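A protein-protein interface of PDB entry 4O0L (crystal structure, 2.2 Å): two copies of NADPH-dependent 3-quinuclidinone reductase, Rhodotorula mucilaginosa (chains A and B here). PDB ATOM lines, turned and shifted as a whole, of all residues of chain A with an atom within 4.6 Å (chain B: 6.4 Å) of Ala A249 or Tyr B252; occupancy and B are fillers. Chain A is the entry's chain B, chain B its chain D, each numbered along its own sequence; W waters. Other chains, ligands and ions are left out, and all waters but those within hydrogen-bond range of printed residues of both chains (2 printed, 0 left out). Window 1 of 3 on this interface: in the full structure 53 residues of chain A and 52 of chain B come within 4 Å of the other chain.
Water W1 lies within hydrogen-bond range of NZ of Lys A247 and SD of Met B26. Water W2 lies within hydrogen-bond range of O of Ala B257 (2.9 Å), N of Ala A248 (3.0 Å), N of Lys A247 (3.4 Å) and SD of Met B26 (3.7 Å).
Ile A211 touches none of the printed residues of chain B. Of chain B, only Tyr B252 comes within 4 Å of Ala A249. Of the printed residues of chain B, Leu A251 touches Val B23. Of the printed residues of chain B, Tyr A252 touches Ala B248 and Ala B249. Printed residues of chain A within 4 Å of Ala B248: Tyr A252 (3.9 Å). Of the printed residues of chain A, Ala B249 touches Tyr A252 (3.9 Å). Of the printed residues of chain A, Tyr B252 touches Ala A248, Ala A249 and Ile A268. Printed residues of chain A within 4 Å of Thr B261: Ile A268 (3.6 Å). Leu B266 touches none of the printed residues of chain A. The nearest residue of chain B that does not touch Ala A249 is Ala B257 (5.2 Å).
The backbone carbonyl oxygen of Met B26 lies within hydrogen-bond range of the backbone NH of Ala B257, 3.1 Å away. NH1 of Arg B207 is in hydrogen-bond range of O of Thr B261, 3.1 Å away. The side-chain hydroxyl (OG) of Ser B258 sits at hydrogen-bond distance from the backbone carbonyl oxygen (O) of Tyr B252. OH of Tyr B252 is in hydrogen-bond range of OG1 of Thr B261 (2.8 Å). The side-chain hydroxyl of Ser B255 sits close to the backbone NH of Ala B257, 3.5 Å away.
Ala A248 touches Tyr B252, and with the chains exchanged Tyr A252 touches Ala B248. Ala A249 touches Tyr B252, and with the chains exchanged Tyr A252 touches Ala B249. Positions printed for both chains: 247, 248, 249, 250, 251, 252, 253 and 266.
CB of Lys A247 touches CG2 of Val B23 (3.9 Å). CG2 of Val B23 touches N of Ala A248, at 3.7 Å. Ala A248 touches Phe B27 (CB to CZ, 3.8 Å). Tyr B252 touches Ala A248 (CE1 to CB, 3.9 Å). Ala A249 touches Tyr B252 (CB to OH, 3.9 Å). Leu A251 touches Val B23. CE1 of Tyr A252 touches N of Ala B249, 3.9 Å away. Ile A268 touches Tyr B252. CD2 of Tyr B260 touches O of Ile A268, at 3.8 Å. CG2 of Ile A268 touches OG1 of Thr B261 (3.6 Å).
Hydrophobic or aromatic side chains of chain A within 4 Å of the printed part of chain B: Ala A248, Ala A249, Leu A251, Tyr A252 and Ile A268. Among the printed residues, no Asp or Glu carboxylate lies within 4 Å of a Lys or Arg side-chain nitrogen of the other chain.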
ATOM      1  N   ILE A 211     -21.807  24.568   5.697  1.00  0.00           N
ATOM      2  CA  ILE A 211     -21.293  23.996   4.458  1.00  0.00           C
ATOM      3  C   ILE A 211     -20.773  22.594   4.822  1.00  0.00           C
ATOM      4  O   ILE A 211     -19.938  22.447   5.718  1.00  0.00           O
ATOM      5  CB  ILE A 211     -20.184  24.869   3.825  1.00  0.00           C
ATOM      6  CG1 ILE A 211     -20.790  26.231   3.413  1.00  0.00           C
ATOM      7  CG2 ILE A 211     -19.583  24.184   2.570  1.00  0.00           C
ATOM      8  CD1 ILE A 211     -19.861  27.147   2.682  1.00  0.00           C
ATOM      9  N   LEU A 246     -14.912  24.973  -3.082  1.00  0.00           N
ATOM     10  CA  LEU A 246     -15.654  25.450  -1.904  1.00  0.00           C
ATOM     11  C   LEU A 246     -15.721  26.974  -1.850  1.00  0.00           C
ATOM     12  O   LEU A 246     -16.655  27.543  -1.273  1.00  0.00           O
ATOM     13  CB  LEU A 246     -15.028  24.934  -0.616  1.00  0.00           C
ATOM     14  CG  LEU A 246     -15.161  23.401  -0.461  1.00  0.00           C
ATOM     15  CD1 LEU A 246     -14.228  22.864   0.592  1.00  0.00           C
ATOM     16  CD2 LEU A 246     -16.595  23.022  -0.130  1.00  0.00           C
ATOM     17  N   LYS A 247     -14.742  27.616  -2.460  1.00  0.00           N
ATOM     18  CA  LYS A 247     -14.570  29.079  -2.347  1.00  0.00           C
ATOM     19  C   LYS A 247     -15.862  29.877  -2.532  1.00  0.00           C
ATOM     20  O   LYS A 247     -16.200  30.702  -1.700  1.00  0.00           O
ATOM     21  CB  LYS A 247     -13.498  29.573  -3.325  1.00  0.00           C
ATOM     22  CG  LYS A 247     -12.114  29.242  -2.884  1.00  0.00           C
ATOM     23  CD  LYS A 247     -11.059  29.573  -3.953  1.00  0.00           C
ATOM     24  CE  LYS A 247     -10.836  31.091  -4.111  1.00  0.00           C
ATOM     25  NZ  LYS A 247      -9.783  31.359  -5.124  1.00  0.00           N
ATOM     26  N   ALA A 248     -16.567  29.592  -3.622  1.00  0.00           N
ATOM     27  CA  ALA A 248     -17.752  30.304  -4.001  1.00  0.00           C
ATOM     28  C   ALA A 248     -18.910  30.102  -3.018  1.00  0.00           C
ATOM     29  O   ALA A 248     -19.725  30.998  -2.834  1.00  0.00           O
ATOM     30  CB  ALA A 248     -18.170  29.914  -5.385  1.00  0.00           C
ATOM     31  N   ALA A 249     -18.959  28.938  -2.386  1.00  0.00           N
ATOM     32  CA  ALA A 249     -19.992  28.644  -1.405  1.00  0.00           C
ATOM     33  C   ALA A 249     -19.798  29.453  -0.130  1.00  0.00           C
ATOM     34  O   ALA A 249     -20.776  29.947   0.438  1.00  0.00           O
ATOM     35  CB  ALA A 249     -20.039  27.127  -1.105  1.00  0.00           C
ATOM     36  N   TYR A 250     -18.539  29.599   0.315  1.00  0.00           N
ATOM     37  CA  TYR A 250     -18.208  30.394   1.522  1.00  0.00           C
ATOM     38  C   TYR A 250     -18.497  31.889   1.290  1.00  0.00           C
ATOM     39  O   TYR A 250     -19.126  32.548   2.129  1.00  0.00           O
ATOM     40  CB  TYR A 250     -16.784  30.170   2.003  1.00  0.00           C
ATOM     41  CG  TYR A 250     -16.623  28.849   2.732  1.00  0.00           C
ATOM     42  CD1 TYR A 250     -16.923  28.731   4.099  1.00  0.00           C
ATOM     43  CD2 TYR A 250     -16.216  27.709   2.056  1.00  0.00           C
ATOM     44  CE1 TYR A 250     -16.813  27.508   4.764  1.00  0.00           C
ATOM     45  CE2 TYR A 250     -16.111  26.494   2.713  1.00  0.00           C
ATOM     46  CZ  TYR A 250     -16.401  26.402   4.063  1.00  0.00           C
ATOM     47  OH  TYR A 250     -16.286  25.178   4.677  1.00  0.00           O
ATOM     48  N   LEU A 251     -18.073  32.380   0.121  1.00  0.00           N
ATOM     49  CA  LEU A 251     -18.374  33.740  -0.297  1.00  0.00           C
ATOM     50  C   LEU A 251     -19.895  33.967  -0.394  1.00  0.00           C
ATOM     51  O   LEU A 251     -20.400  35.003   0.032  1.00  0.00           O
ATOM     52  CB  LEU A 251     -17.722  34.031  -1.654  1.00  0.00           C
ATOM     53  CG  LEU A 251     -17.879  35.478  -2.148  1.00  0.00           C
ATOM     54  CD1 LEU A 251     -17.441  36.490  -1.076  1.00  0.00           C
ATOM     55  CD2 LEU A 251     -17.128  35.690  -3.473  1.00  0.00           C
ATOM     56  N   TYR A 252     -20.609  32.983  -0.954  1.00  0.00           N
ATOM     57  CA  TYR A 252     -22.052  33.059  -1.088  1.00  0.00           C
ATOM     58  C   TYR A 252     -22.713  33.317   0.284  1.00  0.00           C
ATOM     59  O   TYR A 252     -23.513  34.237   0.436  1.00  0.00           O
ATOM     60  CB  TYR A 252     -22.597  31.794  -1.787  1.00  0.00           C
ATOM     61  CG  TYR A 252     -24.115  31.652  -1.745  1.00  0.00           C
ATOM     62  CD1 TYR A 252     -24.928  32.311  -2.676  1.00  0.00           C
ATOM     63  CD2 TYR A 252     -24.728  30.900  -0.751  1.00  0.00           C
ATOM     64  CE1 TYR A 252     -26.299  32.215  -2.614  1.00  0.00           C
ATOM     65  CE2 TYR A 252     -26.117  30.796  -0.668  1.00  0.00           C
ATOM     66  CZ  TYR A 252     -26.898  31.431  -1.591  1.00  0.00           C
ATOM     67  OH  TYR A 252     -28.270  31.304  -1.485  1.00  0.00           O
ATOM     68  N   LEU A 253     -22.326  32.523   1.279  1.00  0.00           N
ATOM     69  CA  LEU A 253     -22.904  32.593   2.614  1.00  0.00           C
ATOM     70  C   LEU A 253     -22.443  33.793   3.424  1.00  0.00           C
ATOM     71  O   LEU A 253     -23.203  34.323   4.240  1.00  0.00           O
ATOM     72  CB  LEU A 253     -22.608  31.320   3.396  1.00  0.00           C
ATOM     73  CG  LEU A 253     -23.352  30.063   2.979  1.00  0.00           C
ATOM     74  CD1 LEU A 253     -22.963  28.953   3.954  1.00  0.00           C
ATOM     75  CD2 LEU A 253     -24.884  30.294   2.955  1.00  0.00           C
ATOM     76  N   LEU A 266     -25.297  23.643   2.996  1.00  0.00           N
ATOM     77  CA  LEU A 266     -24.848  23.497   1.625  1.00  0.00           C
ATOM     78  C   LEU A 266     -24.013  22.238   1.465  1.00  0.00           C
ATOM     79  O   LEU A 266     -22.903  22.168   1.964  1.00  0.00           O
ATOM     80  CB  LEU A 266     -24.035  24.722   1.187  1.00  0.00           C
ATOM     81  CG  LEU A 266     -24.828  25.914   0.660  1.00  0.00           C
ATOM     82  CD1 LEU A 266     -26.089  26.215   1.458  1.00  0.00           C
ATOM     83  CD2 LEU A 266     -23.909  27.117   0.595  1.00  0.00           C
ATOM     84  N   ILE A 268     -21.699  19.932  -0.435  1.00  0.00           N
ATOM     85  CA  ILE A 268     -20.733  20.034  -1.566  1.00  0.00           C
ATOM     86  C   ILE A 268     -19.838  18.812  -1.572  1.00  0.00           C
ATOM     87  O   ILE A 268     -18.753  18.840  -1.026  1.00  0.00           O
ATOM     88  CB  ILE A 268     -19.917  21.335  -1.520  1.00  0.00           C
ATOM     89  CG1 ILE A 268     -20.876  22.541  -1.567  1.00  0.00           C
ATOM     90  CG2 ILE A 268     -18.935  21.381  -2.677  1.00  0.00           C
ATOM     91  CD1 ILE A 268     -20.218  23.867  -1.215  1.00  0.00           C
ATOM     92  N   VAL B  23     -12.213  33.640  -7.759  1.00  0.00           N
ATOM     93  CA  VAL B  23     -13.550  33.130  -7.425  1.00  0.00           C
ATOM     94  C   VAL B  23     -14.606  33.796  -8.289  1.00  0.00           C
ATOM     95  O   VAL B  23     -15.564  33.134  -8.703  1.00  0.00           O
ATOM     96  CB  VAL B  23     -13.877  33.241  -5.903  1.00  0.00           C
ATOM     97  CG1 VAL B  23     -14.054  34.694  -5.446  1.00  0.00           C
ATOM     98  CG2 VAL B  23     -15.104  32.391  -5.518  1.00  0.00           C
ATOM     99  N   MET B  26     -14.889  32.204 -11.655  1.00  0.00           N
ATOM    100  CA  MET B  26     -15.624  30.929 -11.595  1.00  0.00           C
ATOM    101  C   MET B  26     -17.115  31.097 -11.945  1.00  0.00           C
ATOM    102  O   MET B  26     -17.738  30.182 -12.446  1.00  0.00           O
ATOM    103  CB  MET B  26     -15.493  30.292 -10.200  1.00  0.00           C
ATOM    104  CG  MET B  26     -14.078  30.032  -9.727  1.00  0.00           C
ATOM    105  SD  MET B  26     -14.030  29.150  -8.140  1.00  0.00           S
ATOM    106  CE  MET B  26     -13.769  27.480  -8.718  1.00  0.00           C
ATOM    107  N   PHE B  27     -17.651  32.287 -11.674  1.00  0.00           N
ATOM    108  CA  PHE B  27     -19.059  32.608 -11.901  1.00  0.00           C
ATOM    109  C   PHE B  27     -19.365  33.010 -13.330  1.00  0.00           C
ATOM    110  O   PHE B  27     -20.539  33.152 -13.688  1.00  0.00           O
ATOM    111  CB  PHE B  27     -19.477  33.757 -11.001  1.00  0.00           C
ATOM    112  CG  PHE B  27     -19.702  33.368  -9.578  1.00  0.00           C
ATOM    113  CD1 PHE B  27     -20.893  32.749  -9.204  1.00  0.00           C
ATOM    114  CD2 PHE B  27     -18.765  33.662  -8.610  1.00  0.00           C
ATOM    115  CE1 PHE B  27     -21.138  32.414  -7.865  1.00  0.00           C
ATOM    116  CE2 PHE B  27     -18.989  33.331  -7.259  1.00  0.00           C
ATOM    117  CZ  PHE B  27     -20.182  32.701  -6.891  1.00  0.00           C
ATOM    118  N   ILE B 165     -30.643  22.520 -13.633  1.00  0.00           N
ATOM    119  CA  ILE B 165     -31.137  23.114 -12.420  1.00  0.00           C
ATOM    120  C   ILE B 165     -32.673  23.027 -12.465  1.00  0.00           C
ATOM    121  O   ILE B 165     -33.285  23.365 -13.463  1.00  0.00           O
ATOM    122  CB  ILE B 165     -30.663  24.593 -12.271  1.00  0.00           C
ATOM    123  CG1 ILE B 165     -29.133  24.711 -12.393  1.00  0.00           C
ATOM    124  CG2 ILE B 165     -31.108  25.172 -10.945  1.00  0.00           C
ATOM    125  CD1 ILE B 165     -28.609  26.134 -12.550  1.00  0.00           C
ATOM    126  N   ARG B 207     -23.695  18.033 -14.148  1.00  0.00           N
ATOM    127  CA  ARG B 207     -24.105  18.191 -12.777  1.00  0.00           C
ATOM    128  C   ARG B 207     -25.594  18.548 -12.740  1.00  0.00           C
ATOM    129  O   ARG B 207     -26.108  19.175 -13.675  1.00  0.00           O
ATOM    130  CB  ARG B 207     -23.280  19.255 -12.087  1.00  0.00           C
ATOM    131  CG  ARG B 207     -21.811  18.916 -11.889  1.00  0.00           C
ATOM    132  CD  ARG B 207     -21.098  20.035 -11.147  1.00  0.00           C
ATOM    133  NE  ARG B 207     -21.128  21.292 -11.882  1.00  0.00           N
ATOM    134  CZ  ARG B 207     -21.871  22.348 -11.595  1.00  0.00           C
ATOM    135  NH1 ARG B 207     -22.703  22.325 -10.537  1.00  0.00           N
ATOM    136  NH2 ARG B 207     -21.797  23.438 -12.362  1.00  0.00           N
ATOM    137  N   LYS B 247     -30.900  35.082  -7.053  1.00  0.00           N
ATOM    138  CA  LYS B 247     -30.080  35.242  -8.255  1.00  0.00           C
ATOM    139  C   LYS B 247     -28.710  34.599  -8.156  1.00  0.00           C
ATOM    140  O   LYS B 247     -28.216  34.004  -9.119  1.00  0.00           O
ATOM    141  CB  LYS B 247     -29.910  36.710  -8.614  1.00  0.00           C
ATOM    142  CG  LYS B 247     -31.146  37.358  -9.182  1.00  0.00           C
ATOM    143  CD  LYS B 247     -30.960  38.858  -9.366  1.00  0.00           C
ATOM    144  CE  LYS B 247     -29.948  39.172 -10.444  1.00  0.00           C
ATOM    145  NZ  LYS B 247     -29.738  40.656 -10.489  1.00  0.00           N
ATOM    146  N   ALA B 248     -28.092  34.727  -6.984  1.00  0.00           N
ATOM    147  CA  ALA B 248     -26.743  34.261  -6.776  1.00  0.00           C
ATOM    148  C   ALA B 248     -26.682  32.734  -6.778  1.00  0.00           C
ATOM    149  O   ALA B 248     -25.708  32.161  -7.267  1.00  0.00           O
ATOM    150  CB  ALA B 248     -26.209  34.808  -5.496  1.00  0.00           C
ATOM    151  N   ALA B 249     -27.730  32.103  -6.247  1.00  0.00           N
ATOM    152  CA  ALA B 249     -27.827  30.634  -6.174  1.00  0.00           C
ATOM    153  C   ALA B 249     -27.952  29.994  -7.555  1.00  0.00           C
ATOM    154  O   ALA B 249     -27.330  28.953  -7.824  1.00  0.00           O
ATOM    155  CB  ALA B 249     -28.997  30.231  -5.298  1.00  0.00           C
ATOM    156  N   TYR B 250     -28.742  30.609  -8.447  1.00  0.00           N
ATOM    157  CA  TYR B 250     -28.825  30.129  -9.828  1.00  0.00           C
ATOM    158  C   TYR B 250     -27.497  30.320 -10.580  1.00  0.00           C
ATOM    159  O   TYR B 250     -27.068  29.453 -11.312  1.00  0.00           O
ATOM    160  CB  TYR B 250     -29.995  30.768 -10.586  1.00  0.00           C
ATOM    161  CG  TYR B 250     -31.346  30.265 -10.149  1.00  0.00           C
ATOM    162  CD1 TYR B 250     -31.883  29.079 -10.673  1.00  0.00           C
ATOM    163  CD2 TYR B 250     -32.084  30.957  -9.196  1.00  0.00           C
ATOM    164  CE1 TYR B 250     -33.139  28.613 -10.266  1.00  0.00           C
ATOM    165  CE2 TYR B 250     -33.339  30.480  -8.759  1.00  0.00           C
ATOM    166  CZ  TYR B 250     -33.844  29.310  -9.295  1.00  0.00           C
ATOM    167  OH  TYR B 250     -35.064  28.862  -8.862  1.00  0.00           O
ATOM    168  N   LEU B 251     -26.862  31.465 -10.404  1.00  0.00           N
ATOM    169  CA  LEU B 251     -25.571  31.711 -11.064  1.00  0.00           C
ATOM    170  C   LEU B 251     -24.515  30.719 -10.512  1.00  0.00           C
ATOM    171  O   LEU B 251     -23.682  30.226 -11.237  1.00  0.00           O
ATOM    172  CB  LEU B 251     -25.103  33.131 -10.806  1.00  0.00           C
ATOM    173  CG  LEU B 251     -24.280  33.886 -11.858  1.00  0.00           C
ATOM    174  CD1 LEU B 251     -23.454  34.975 -11.188  1.00  0.00           C
ATOM    175  CD2 LEU B 251     -23.421  32.974 -12.721  1.00  0.00           C
ATOM    176  N   TYR B 252     -24.562  30.484  -9.200  1.00  0.00           N
ATOM    177  CA  TYR B 252     -23.668  29.545  -8.531  1.00  0.00           C
ATOM    178  C   TYR B 252     -23.750  28.139  -9.163  1.00  0.00           C
ATOM    179  O   TYR B 252     -22.736  27.550  -9.506  1.00  0.00           O
ATOM    180  CB  TYR B 252     -23.962  29.502  -7.034  1.00  0.00           C
ATOM    181  CG  TYR B 252     -23.239  28.399  -6.297  1.00  0.00           C
ATOM    182  CD1 TYR B 252     -21.897  28.514  -5.949  1.00  0.00           C
ATOM    183  CD2 TYR B 252     -23.913  27.204  -5.955  1.00  0.00           C
ATOM    184  CE1 TYR B 252     -21.233  27.479  -5.311  1.00  0.00           C
ATOM    185  CE2 TYR B 252     -23.261  26.178  -5.317  1.00  0.00           C
ATOM    186  CZ  TYR B 252     -21.944  26.306  -4.974  1.00  0.00           C
ATOM    187  OH  TYR B 252     -21.322  25.256  -4.329  1.00  0.00           O
ATOM    188  N   LEU B 253     -24.963  27.635  -9.346  1.00  0.00           N
ATOM    189  CA  LEU B 253     -25.156  26.310  -9.920  1.00  0.00           C
ATOM    190  C   LEU B 253     -24.870  26.213 -11.426  1.00  0.00           C
ATOM    191  O   LEU B 253     -24.413  25.164 -11.924  1.00  0.00           O
ATOM    192  CB  LEU B 253     -26.560  25.797  -9.624  1.00  0.00           C
ATOM    193  CG  LEU B 253     -26.875  25.514  -8.156  1.00  0.00           C
ATOM    194  CD1 LEU B 253     -28.314  25.107  -8.048  1.00  0.00           C
ATOM    195  CD2 LEU B 253     -25.967  24.433  -7.568  1.00  0.00           C
ATOM    196  N   ALA B 254     -25.125  27.316 -12.126  1.00  0.00           N
ATOM    197  CA  ALA B 254     -25.030  27.370 -13.591  1.00  0.00           C
ATOM    198  C   ALA B 254     -23.577  27.419 -14.046  1.00  0.00           C
ATOM    199  O   ALA B 254     -23.273  27.053 -15.167  1.00  0.00           O
ATOM    200  CB  ALA B 254     -25.791  28.590 -14.133  1.00  0.00           C
ATOM    201  N   SER B 255     -22.711  27.884 -13.154  1.00  0.00           N
ATOM    202  CA  SER B 255     -21.327  28.181 -13.490  1.00  0.00           C
ATOM    203  C   SER B 255     -20.305  27.206 -12.889  1.00  0.00           C
ATOM    204  O   SER B 255     -20.659  26.238 -12.217  1.00  0.00           O
ATOM    205  CB  SER B 255     -21.006  29.635 -13.085  1.00  0.00           C
ATOM    206  OG  SER B 255     -21.138  29.801 -11.692  1.00  0.00           O
ATOM    207  N   ASN B 256     -19.037  27.474 -13.159  1.00  0.00           N
ATOM    208  CA  ASN B 256     -17.910  26.758 -12.538  1.00  0.00           C
ATOM    209  C   ASN B 256     -17.639  27.127 -11.071  1.00  0.00           C
ATOM    210  O   ASN B 256     -16.689  26.653 -10.467  1.00  0.00           O
ATOM    211  CB  ASN B 256     -16.639  26.924 -13.390  1.00  0.00           C
ATOM    212  CG  ASN B 256     -16.698  26.165 -14.693  1.00  0.00           C
ATOM    213  OD1 ASN B 256     -17.558  25.316 -14.893  1.00  0.00           O
ATOM    214  ND2 ASN B 256     -15.779  26.469 -15.596  1.00  0.00           N
ATOM    215  N   ALA B 257     -18.482  27.958 -10.487  1.00  0.00           N
ATOM    216  CA  ALA B 257     -18.446  28.202  -9.046  1.00  0.00           C
ATOM    217  C   ALA B 257     -18.778  26.921  -8.254  1.00  0.00           C
ATOM    218  O   ALA B 257     -18.451  26.828  -7.061  1.00  0.00           O
ATOM    219  CB  ALA B 257     -19.427  29.307  -8.665  1.00  0.00           C
ATOM    220  N   SER B 258     -19.402  25.938  -8.903  1.00  0.00           N
ATOM    221  CA  SER B 258     -19.932  24.770  -8.194  1.00  0.00           C
ATOM    222  C   SER B 258     -19.567  23.401  -8.782  1.00  0.00           C
ATOM    223  O   SER B 258     -20.397  22.487  -8.791  1.00  0.00           O
ATOM    224  CB  SER B 258     -21.450  24.879  -8.063  1.00  0.00           C
ATOM    225  OG  SER B 258     -22.084  24.974  -9.310  1.00  0.00           O
ATOM    226  N   THR B 259     -18.333  23.243  -9.228  1.00  0.00           N
ATOM    227  CA  THR B 259     -17.965  22.038  -9.985  1.00  0.00           C
ATOM    228  C   THR B 259     -17.939  20.725  -9.162  1.00  0.00           C
ATOM    229  O   THR B 259     -17.863  19.647  -9.739  1.00  0.00           O
ATOM    230  CB  THR B 259     -16.630  22.212 -10.751  1.00  0.00           C
ATOM    231  OG1 THR B 259     -15.632  22.662  -9.854  1.00  0.00           O
ATOM    232  CG2 THR B 259     -16.777  23.253 -11.872  1.00  0.00           C
ATOM    233  N   TYR B 260     -17.982  20.814  -7.840  1.00  0.00           N
ATOM    234  CA  TYR B 260     -18.056  19.630  -7.009  1.00  0.00           C
ATOM    235  C   TYR B 260     -19.435  19.535  -6.313  1.00  0.00           C
ATOM    236  O   TYR B 260     -19.643  18.707  -5.415  1.00  0.00           O
ATOM    237  CB  TYR B 260     -16.910  19.605  -6.005  1.00  0.00           C
ATOM    238  CG  TYR B 260     -16.569  18.220  -5.459  1.00  0.00           C
ATOM    239  CD1 TYR B 260     -16.030  17.216  -6.281  1.00  0.00           C
ATOM    240  CD2 TYR B 260     -16.719  17.942  -4.093  1.00  0.00           C
ATOM    241  CE1 TYR B 260     -15.672  15.947  -5.742  1.00  0.00           C
ATOM    242  CE2 TYR B 260     -16.362  16.702  -3.565  1.00  0.00           C
ATOM    243  CZ  TYR B 260     -15.873  15.693  -4.392  1.00  0.00           C
ATOM    244  OH  TYR B 260     -15.576  14.471  -3.812  1.00  0.00           O
ATOM    245  N   THR B 261     -20.361  20.371  -6.762  1.00  0.00           N
ATOM    246  CA  THR B 261     -21.722  20.400  -6.217  1.00  0.00           C
ATOM    247  C   THR B 261     -22.690  19.713  -7.197  1.00  0.00           C
ATOM    248  O   THR B 261     -23.040  20.244  -8.265  1.00  0.00           O
ATOM    249  CB  THR B 261     -22.188  21.857  -5.934  1.00  0.00           C
ATOM    250  OG1 THR B 261     -21.166  22.577  -5.194  1.00  0.00           O
ATOM    251  CG2 THR B 261     -23.511  21.864  -5.113  1.00  0.00           C
ATOM    252  N   LEU B 266     -30.443  23.375  -2.739  1.00  0.00           N
ATOM    253  CA  LEU B 266     -30.240  24.671  -2.081  1.00  0.00           C
ATOM    254  C   LEU B 266     -31.576  25.219  -1.537  1.00  0.00           C
ATOM    255  O   LEU B 266     -32.458  25.593  -2.295  1.00  0.00           O
ATOM    256  CB  LEU B 266     -29.629  25.688  -3.075  1.00  0.00           C
ATOM    257  CG  LEU B 266     -28.121  25.587  -3.369  1.00  0.00           C
ATOM    258  CD1 LEU B 266     -27.712  24.184  -3.757  1.00  0.00           C
ATOM    259  CD2 LEU B 266     -27.707  26.570  -4.445  1.00  0.00           C
HETATM  260  O   HOH W   1     -10.940  30.273  -7.288  1.00  0.00           O
HETATM  261  O   HOH W   2     -15.998  27.432  -5.578  1.00  0.00           O
